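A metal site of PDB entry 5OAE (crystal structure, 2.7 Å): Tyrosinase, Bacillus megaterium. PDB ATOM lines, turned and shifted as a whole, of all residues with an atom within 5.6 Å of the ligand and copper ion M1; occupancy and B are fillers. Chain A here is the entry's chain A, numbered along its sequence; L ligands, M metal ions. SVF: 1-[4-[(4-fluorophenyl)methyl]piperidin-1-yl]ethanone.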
ATOM      1  N   HIS A  39     -10.729 -21.920  11.903  1.00  0.00           N
ATOM      2  CA  HIS A  39     -10.069 -21.866  10.610  1.00  0.00           C
ATOM      3  C   HIS A  39     -10.961 -21.234   9.554  1.00  0.00           C
ATOM      4  O   HIS A  39     -10.519 -20.376   8.785  1.00  0.00           O
ATOM      5  CB  HIS A  39      -9.650 -23.274  10.171  1.00  0.00           C
ATOM      6  CG  HIS A  39      -8.851 -23.300   8.910  1.00  0.00           C
ATOM      7  ND1 HIS A  39      -9.385 -23.659   7.694  1.00  0.00           N
ATOM      8  CD2 HIS A  39      -7.541 -23.049   8.681  1.00  0.00           C
ATOM      9  CE1 HIS A  39      -8.445 -23.604   6.765  1.00  0.00           C
ATOM     10  NE2 HIS A  39      -7.319 -23.236   7.339  1.00  0.00           N
ATOM     11  N   ALA A  56      -6.078 -15.659   7.986  1.00  0.00           N
ATOM     12  CA  ALA A  56      -5.307 -16.890   8.045  1.00  0.00           C
ATOM     13  C   ALA A  56      -4.613 -17.241   6.739  1.00  0.00           C
ATOM     14  O   ALA A  56      -3.686 -18.059   6.728  1.00  0.00           O
ATOM     15  CB  ALA A  56      -6.211 -18.037   8.471  1.00  0.00           C
ATOM     16  N   HIS A  57      -5.052 -16.647   5.633  1.00  0.00           N
ATOM     17  CA  HIS A  57      -4.519 -17.037   4.329  1.00  0.00           C
ATOM     18  C   HIS A  57      -4.293 -15.869   3.374  1.00  0.00           C
ATOM     19  O   HIS A  57      -4.753 -14.751   3.615  1.00  0.00           O
ATOM     20  CB  HIS A  57      -5.450 -18.043   3.655  1.00  0.00           C
ATOM     21  CG  HIS A  57      -5.816 -19.212   4.531  1.00  0.00           C
ATOM     22  ND1 HIS A  57      -6.954 -19.232   5.302  1.00  0.00           N
ATOM     23  CD2 HIS A  57      -5.179 -20.384   4.754  1.00  0.00           C
ATOM     24  CE1 HIS A  57      -7.011 -20.376   5.960  1.00  0.00           C
ATOM     25  NE2 HIS A  57      -5.949 -21.096   5.652  1.00  0.00           N
ATOM     26  N   PHE A  62      -0.128 -15.771   7.193  1.00  0.00           N
ATOM     27  CA  PHE A  62      -0.453 -17.167   6.901  1.00  0.00           C
ATOM     28  C   PHE A  62       0.357 -18.142   7.751  1.00  0.00           C
ATOM     29  O   PHE A  62      -0.188 -19.103   8.288  1.00  0.00           O
ATOM     30  CB  PHE A  62      -0.210 -17.465   5.420  1.00  0.00           C
ATOM     31  CG  PHE A  62      -0.072 -18.924   5.111  1.00  0.00           C
ATOM     32  CD1 PHE A  62      -1.171 -19.766   5.139  1.00  0.00           C
ATOM     33  CD2 PHE A  62       1.167 -19.466   4.777  1.00  0.00           C
ATOM     34  CE1 PHE A  62      -1.036 -21.120   4.854  1.00  0.00           C
ATOM     35  CE2 PHE A  62       1.304 -20.803   4.492  1.00  0.00           C
ATOM     36  CZ  PHE A  62       0.206 -21.634   4.529  1.00  0.00           C
ATOM     37  N   TRP A  65      -0.147 -17.636  11.880  1.00  0.00           N
ATOM     38  CA  TRP A  65      -1.505 -18.022  12.253  1.00  0.00           C
ATOM     39  C   TRP A  65      -1.567 -19.528  12.480  1.00  0.00           C
ATOM     40  O   TRP A  65      -2.023 -19.992  13.516  1.00  0.00           O
ATOM     41  CB  TRP A  65      -2.506 -17.610  11.177  1.00  0.00           C
ATOM     42  CG  TRP A  65      -3.940 -17.703  11.603  1.00  0.00           C
ATOM     43  CD1 TRP A  65      -4.723 -16.679  12.073  1.00  0.00           C
ATOM     44  CD2 TRP A  65      -4.775 -18.870  11.589  1.00  0.00           C
ATOM     45  NE1 TRP A  65      -5.988 -17.150  12.359  1.00  0.00           N
ATOM     46  CE2 TRP A  65      -6.042 -18.478  12.072  1.00  0.00           C
ATOM     47  CE3 TRP A  65      -4.571 -20.203  11.229  1.00  0.00           C
ATOM     48  CZ2 TRP A  65      -7.095 -19.389  12.192  1.00  0.00           C
ATOM     49  CZ3 TRP A  65      -5.622 -21.098  11.349  1.00  0.00           C
ATOM     50  CH2 TRP A  65      -6.865 -20.678  11.829  1.00  0.00           C
ATOM     51  N   HIS A  66      -1.100 -20.279  11.491  1.00  0.00           N
ATOM     52  CA  HIS A  66      -1.164 -21.731  11.546  1.00  0.00           C
ATOM     53  C   HIS A  66      -0.194 -22.302  12.580  1.00  0.00           C
ATOM     54  O   HIS A  66      -0.418 -23.391  13.097  1.00  0.00           O
ATOM     55  CB  HIS A  66      -0.894 -22.324  10.167  1.00  0.00           C
ATOM     56  CG  HIS A  66      -2.003 -22.081   9.192  1.00  0.00           C
ATOM     57  ND1 HIS A  66      -2.078 -20.938   8.420  1.00  0.00           N
ATOM     58  CD2 HIS A  66      -3.094 -22.827   8.870  1.00  0.00           C
ATOM     59  CE1 HIS A  66      -3.163 -20.996   7.652  1.00  0.00           C
ATOM     60  NE2 HIS A  66      -3.789 -22.131   7.907  1.00  0.00           N
ATOM     61  N   GLY A 193       1.966 -21.082  -1.749  1.00  0.00           N
ATOM     62  CA  GLY A 193       1.824 -21.769  -3.020  1.00  0.00           C
ATOM     63  C   GLY A 193       1.090 -21.009  -4.102  1.00  0.00           C
ATOM     64  O   GLY A 193       0.422 -21.618  -4.945  1.00  0.00           O
ATOM     65  N   PHE A 194       1.188 -19.683  -4.096  1.00  0.00           N
ATOM     66  CA  PHE A 194       0.506 -18.883  -5.107  1.00  0.00           C
ATOM     67  C   PHE A 194       1.439 -18.518  -6.258  1.00  0.00           C
ATOM     68  O   PHE A 194       0.996 -17.995  -7.279  1.00  0.00           O
ATOM     69  CB  PHE A 194      -0.101 -17.631  -4.466  1.00  0.00           C
ATOM     70  CG  PHE A 194      -1.272 -17.920  -3.583  1.00  0.00           C
ATOM     71  CD1 PHE A 194      -2.468 -18.386  -4.111  1.00  0.00           C
ATOM     72  CD2 PHE A 194      -1.188 -17.721  -2.211  1.00  0.00           C
ATOM     73  CE1 PHE A 194      -3.549 -18.650  -3.299  1.00  0.00           C
ATOM     74  CE2 PHE A 194      -2.270 -17.992  -1.390  1.00  0.00           C
ATOM     75  CZ  PHE A 194      -3.457 -18.452  -1.939  1.00  0.00           C
ATOM     76  N   GLY A 197       0.722 -21.151  -8.833  1.00  0.00           N
ATOM     77  CA  GLY A 197      -0.009 -22.110  -8.045  1.00  0.00           C
ATOM     78  C   GLY A 197      -0.891 -23.038  -8.868  1.00  0.00           C
ATOM     79  O   GLY A 197      -1.131 -22.786 -10.047  1.00  0.00           O
ATOM     80  N   PRO A 198      -1.372 -24.100  -8.236  1.00  0.00           N
ATOM     81  CA  PRO A 198      -1.064 -24.374  -6.831  1.00  0.00           C
ATOM     82  C   PRO A 198       0.283 -25.072  -6.671  1.00  0.00           C
ATOM     83  O   PRO A 198       0.625 -25.940  -7.474  1.00  0.00           O
ATOM     84  CB  PRO A 198      -2.193 -25.303  -6.399  1.00  0.00           C
ATOM     85  CG  PRO A 198      -2.602 -26.007  -7.650  1.00  0.00           C
ATOM     86  CD  PRO A 198      -2.424 -24.995  -8.758  1.00  0.00           C
ATOM     87  N   GLN A 199       1.030 -24.723  -5.648  1.00  0.00           N
ATOM     88  CA  GLN A 199       2.301 -25.379  -5.406  1.00  0.00           C
ATOM     89  C   GLN A 199       2.551 -25.513  -3.919  1.00  0.00           C
ATOM     90  O   GLN A 199       1.985 -24.812  -3.138  1.00  0.00           O
ATOM     91  CB  GLN A 199       3.430 -24.656  -6.108  1.00  0.00           C
ATOM     92  CG  GLN A 199       3.139 -24.366  -7.562  1.00  0.00           C
ATOM     93  CD  GLN A 199       3.724 -25.388  -8.496  1.00  0.00           C
ATOM     94  OE1 GLN A 199       4.437 -26.279  -8.077  1.00  0.00           O
ATOM     95  NE2 GLN A 199       3.415 -25.272  -9.767  1.00  0.00           N
ATOM     96  N   HIS A 201       2.352 -26.036  -0.257  1.00  0.00           N
ATOM     97  CA  HIS A 201       1.201 -26.073   0.649  1.00  0.00           C
ATOM     98  C   HIS A 201      -0.139 -26.114  -0.086  1.00  0.00           C
ATOM     99  O   HIS A 201      -0.984 -26.957   0.216  1.00  0.00           O
ATOM    100  CB  HIS A 201       1.249 -24.866   1.588  1.00  0.00           C
ATOM    101  CG  HIS A 201      -0.063 -24.563   2.249  1.00  0.00           C
ATOM    102  ND1 HIS A 201      -0.905 -23.570   1.802  1.00  0.00           N
ATOM    103  CD2 HIS A 201      -0.664 -25.104   3.325  1.00  0.00           C
ATOM    104  CE1 HIS A 201      -1.970 -23.517   2.572  1.00  0.00           C
ATOM    105  NE2 HIS A 201      -1.855 -24.439   3.506  1.00  0.00           N
ATOM    106  N   ASN A 202      -0.335 -25.212  -1.043  1.00  0.00           N
ATOM    107  CA  ASN A 202      -1.584 -25.141  -1.787  1.00  0.00           C
ATOM    108  C   ASN A 202      -1.815 -26.373  -2.655  1.00  0.00           C
ATOM    109  O   ASN A 202      -2.949 -26.820  -2.830  1.00  0.00           O
ATOM    110  CB  ASN A 202      -1.628 -23.879  -2.655  1.00  0.00           C
ATOM    111  CG  ASN A 202      -1.834 -22.620  -1.842  1.00  0.00           C
ATOM    112  OD1 ASN A 202      -2.213 -22.675  -0.667  1.00  0.00           O
ATOM    113  ND2 ASN A 202      -1.599 -21.461  -2.457  1.00  0.00           N
ATOM    114  N   ARG A 203      -0.733 -26.913  -3.202  1.00  0.00           N
ATOM    115  CA  ARG A 203      -0.809 -28.094  -4.053  1.00  0.00           C
ATOM    116  C   ARG A 203      -1.194 -29.336  -3.267  1.00  0.00           C
ATOM    117  O   ARG A 203      -1.950 -30.177  -3.742  1.00  0.00           O
ATOM    118  CB  ARG A 203       0.527 -28.324  -4.769  1.00  0.00           C
ATOM    119  CG  ARG A 203       0.591 -29.584  -5.612  1.00  0.00           C
ATOM    120  CD  ARG A 203       1.900 -29.683  -6.361  1.00  0.00           C
ATOM    121  NE  ARG A 203       1.960 -28.778  -7.510  1.00  0.00           N
ATOM    122  CZ  ARG A 203       1.759 -29.151  -8.761  1.00  0.00           C
ATOM    123  NH1 ARG A 203       1.505 -30.421  -9.042  1.00  0.00           N
ATOM    124  NH2 ARG A 203       1.827 -28.261  -9.746  1.00  0.00           N
ATOM    125  N   HIS A 205      -3.055 -29.472  -0.589  1.00  0.00           N
ATOM    126  CA  HIS A 205      -4.491 -29.378  -0.325  1.00  0.00           C
ATOM    127  C   HIS A 205      -5.273 -29.907  -1.518  1.00  0.00           C
ATOM    128  O   HIS A 205      -6.138 -30.782  -1.376  1.00  0.00           O
ATOM    129  CB  HIS A 205      -4.901 -27.935  -0.033  1.00  0.00           C
ATOM    130  CG  HIS A 205      -4.686 -27.513   1.390  1.00  0.00           C
ATOM    131  ND1 HIS A 205      -5.482 -27.962   2.423  1.00  0.00           N
ATOM    132  CD2 HIS A 205      -3.773 -26.691   1.956  1.00  0.00           C
ATOM    133  CE1 HIS A 205      -5.062 -27.439   3.559  1.00  0.00           C
ATOM    134  NE2 HIS A 205      -4.027 -26.663   3.304  1.00  0.00           N
ATOM    135  N   ARG A 206      -4.995 -29.352  -2.694  1.00  0.00           N
ATOM    136  CA  ARG A 206      -5.690 -29.746  -3.916  1.00  0.00           C
ATOM    137  C   ARG A 206      -5.449 -31.198  -4.296  1.00  0.00           C
ATOM    138  O   ARG A 206      -6.305 -31.835  -4.896  1.00  0.00           O
ATOM    139  CB  ARG A 206      -5.279 -28.823  -5.074  1.00  0.00           C
ATOM    140  CG  ARG A 206      -5.613 -27.358  -4.844  1.00  0.00           C
ATOM    141  CD  ARG A 206      -6.658 -26.866  -5.844  1.00  0.00           C
ATOM    142  NE  ARG A 206      -6.316 -25.563  -6.394  1.00  0.00           N
ATOM    143  CZ  ARG A 206      -6.816 -25.079  -7.523  1.00  0.00           C
ATOM    144  NH1 ARG A 206      -7.684 -25.789  -8.225  1.00  0.00           N
ATOM    145  NH2 ARG A 206      -6.439 -23.874  -7.953  1.00  0.00           N
ATOM    146  N   MET A 212     -10.258 -31.306   2.043  1.00  0.00           N
ATOM    147  CA  MET A 212      -8.959 -30.655   2.000  1.00  0.00           C
ATOM    148  C   MET A 212      -8.812 -29.765   0.764  1.00  0.00           C
ATOM    149  O   MET A 212      -7.868 -28.987   0.660  1.00  0.00           O
ATOM    150  CB  MET A 212      -7.837 -31.692   2.015  1.00  0.00           C
ATOM    151  CG  MET A 212      -7.630 -32.379   3.350  1.00  0.00           C
ATOM    152  SD  MET A 212      -6.647 -31.401   4.515  1.00  0.00           S
ATOM    153  CE  MET A 212      -5.112 -31.239   3.606  1.00  0.00           C
ATOM    154  N   GLY A 213      -9.763 -29.871  -0.159  1.00  0.00           N
ATOM    155  CA  GLY A 213      -9.681 -29.120  -1.402  1.00  0.00           C
ATOM    156  C   GLY A 213     -10.130 -27.682  -1.241  1.00  0.00           C
ATOM    157  O   GLY A 213      -9.752 -26.823  -2.041  1.00  0.00           O
ATOM    158  N   VAL A 214     -10.923 -27.406  -0.208  1.00  0.00           N
ATOM    159  CA  VAL A 214     -11.393 -26.060   0.045  1.00  0.00           C
ATOM    160  C   VAL A 214     -11.021 -25.580   1.453  1.00  0.00           C
ATOM    161  O   VAL A 214     -10.820 -26.383   2.358  1.00  0.00           O
ATOM    162  CB  VAL A 214     -12.933 -25.950  -0.148  1.00  0.00           C
ATOM    163  CG1 VAL A 214     -13.333 -26.485  -1.512  1.00  0.00           C
ATOM    164  CG2 VAL A 214     -13.651 -26.699   0.952  1.00  0.00           C
ATOM    165  N   VAL A 215     -10.915 -24.263   1.615  1.00  0.00           N
ATOM    166  CA  VAL A 215     -10.456 -23.681   2.871  1.00  0.00           C
ATOM    167  C   VAL A 215     -11.363 -23.928   4.098  1.00  0.00           C
ATOM    168  O   VAL A 215     -10.881 -24.409   5.116  1.00  0.00           O
ATOM    169  CB  VAL A 215     -10.251 -22.151   2.714  1.00  0.00           C
ATOM    170  CG1 VAL A 215      -9.818 -21.526   4.035  1.00  0.00           C
ATOM    171  CG2 VAL A 215      -9.230 -21.872   1.622  1.00  0.00           C
ATOM    172  N   ALA A 218     -11.405 -27.768   5.276  1.00  0.00           N
ATOM    173  CA  ALA A 218     -10.133 -28.486   5.290  1.00  0.00           C
ATOM    174  C   ALA A 218      -9.799 -29.186   6.629  1.00  0.00           C
ATOM    175  O   ALA A 218      -9.328 -30.325   6.622  1.00  0.00           O
ATOM    176  CB  ALA A 218      -9.005 -27.551   4.899  1.00  0.00           C
ATOM    177  N   PHE A 224      -4.862 -32.596   7.896  1.00  0.00           N
ATOM    178  CA  PHE A 224      -4.669 -31.153   7.812  1.00  0.00           C
ATOM    179  C   PHE A 224      -3.616 -30.681   8.810  1.00  0.00           C
ATOM    180  O   PHE A 224      -2.863 -29.752   8.546  1.00  0.00           O
ATOM    181  CB  PHE A 224      -6.005 -30.425   8.058  1.00  0.00           C
ATOM    182  CG  PHE A 224      -5.907 -28.925   8.029  1.00  0.00           C
ATOM    183  CD1 PHE A 224      -6.054 -28.235   6.839  1.00  0.00           C
ATOM    184  CD2 PHE A 224      -5.686 -28.205   9.196  1.00  0.00           C
ATOM    185  CE1 PHE A 224      -5.970 -26.856   6.809  1.00  0.00           C
ATOM    186  CE2 PHE A 224      -5.602 -26.826   9.166  1.00  0.00           C
ATOM    187  CZ  PHE A 224      -5.744 -26.148   7.980  1.00  0.00           C
ATOM    188  N   HIS A 228       0.201 -29.153   7.898  1.00  0.00           N
ATOM    189  CA  HIS A 228       0.669 -27.838   8.334  1.00  0.00           C
ATOM    190  C   HIS A 228       1.838 -27.925   9.303  1.00  0.00           C
ATOM    191  O   HIS A 228       2.588 -26.965   9.468  1.00  0.00           O
ATOM    192  CB  HIS A 228      -0.487 -27.046   8.953  1.00  0.00           C
ATOM    193  CG  HIS A 228      -1.354 -26.371   7.944  1.00  0.00           C
ATOM    194  ND1 HIS A 228      -1.096 -25.094   7.478  1.00  0.00           N
ATOM    195  CD2 HIS A 228      -2.454 -26.788   7.289  1.00  0.00           C
ATOM    196  CE1 HIS A 228      -2.005 -24.764   6.587  1.00  0.00           C
ATOM    197  NE2 HIS A 228      -2.848 -25.778   6.460  1.00  0.00           N
HETATM  198  C01 SVF L   1      -7.217 -25.067   2.468  1.00  0.00           C
HETATM  199  C02 SVF L   1      -6.883 -24.698   3.768  1.00  0.00           C
HETATM  200  C03 SVF L   1      -6.516 -24.526   1.403  1.00  0.00           C
HETATM  201  C04 SVF L   1      -5.864 -23.809   3.961  1.00  0.00           C
HETATM  202  C05 SVF L   1      -5.496 -23.619   1.622  1.00  0.00           C
HETATM  203  C06 SVF L   1      -5.170 -23.255   2.917  1.00  0.00           C
HETATM  204  C08 SVF L   1      -6.876 -24.833   0.009  1.00  0.00           C
HETATM  205  C09 SVF L   1      -6.515 -23.796  -0.962  1.00  0.00           C
HETATM  206  C10 SVF L   1      -7.526 -23.748  -2.090  1.00  0.00           C
HETATM  207  C11 SVF L   1      -5.134 -24.032  -1.543  1.00  0.00           C
HETATM  208  C12 SVF L   1      -7.164 -22.635  -3.056  1.00  0.00           C
HETATM  209  C13 SVF L   1      -4.786 -22.923  -2.501  1.00  0.00           C
HETATM  210  N14 SVF L   1      -5.813 -22.857  -3.556  1.00  0.00           N
HETATM  211  C15 SVF L   1      -5.492 -22.590  -4.847  1.00  0.00           C
HETATM  212  O16 SVF L   1      -6.254 -21.981  -5.571  1.00  0.00           O
HETATM  213  C17 SVF L   1      -4.056 -22.735  -5.282  1.00  0.00           C
HETATM  214  F07 SVF L   1      -5.543 -23.438   5.236  1.00  0.00           F
HETATM  215 CU    CU M   1      -5.456 -22.656   7.000  1.00  0.00          CU
HETATM  216 CU    CU M   2      -3.388 -25.294   4.599  1.00  0.00          CU
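Merely in contact with copper ion M1: Phe 224.
Copper ion M1 is bound by F07 of the ligand, NE2 of His 66, NE2 of His 39 and NE2 of His 57. Copper ion M1 has four donor atoms within binding distance.
Residues that only touch the ligand: Pro 198 (3.4 Å), His 201 (3.2 Å), Asn 202 (3.0 Å), His 205 (3.3 Å), Gly 213 (3.8 Å), Val 214 (3.8 Å), Val 215 (3.5 Å), Ala 218 (3.7 Å), Phe 224 (3.8 Å) and His 228 (3.8 Å). 14 residues have an atom within 4 Å of the ligand: His 39, His 57, His 66, Pro 198, His 201, Asn 202, His 205, Arg 206, Gly 213, Val 214, Val 215, Ala 218, Phe 224 and His 228.
An oxygen (O16) of the ligand sits at hydrogen-bond distance from the guanidinium group (NH2) of Arg 206 (3.0 Å).
A ring nitrogen (ND1) of His 205 is in hydrogen-bond range of the backbone carbonyl oxygen (O) of Met 212, 3.1 Å away. ND1 of His 39 sits close to O of Val 215, at 3.1 Å. ND1 of His 66 sits at hydrogen-bond distance from O of Phe 62 (2.6 Å). The side-chain amide nitrogen (ND2) of Asn 202 sits close to the backbone carbonyl oxygen (O) of Gly 193 (3.2 Å). O of Pro 198 is in hydrogen-bond range of NE of Arg 203 (3.1 Å). OD1 of Asn 202 is in hydrogen-bond range of ND1 of His 201 (2.9 Å).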
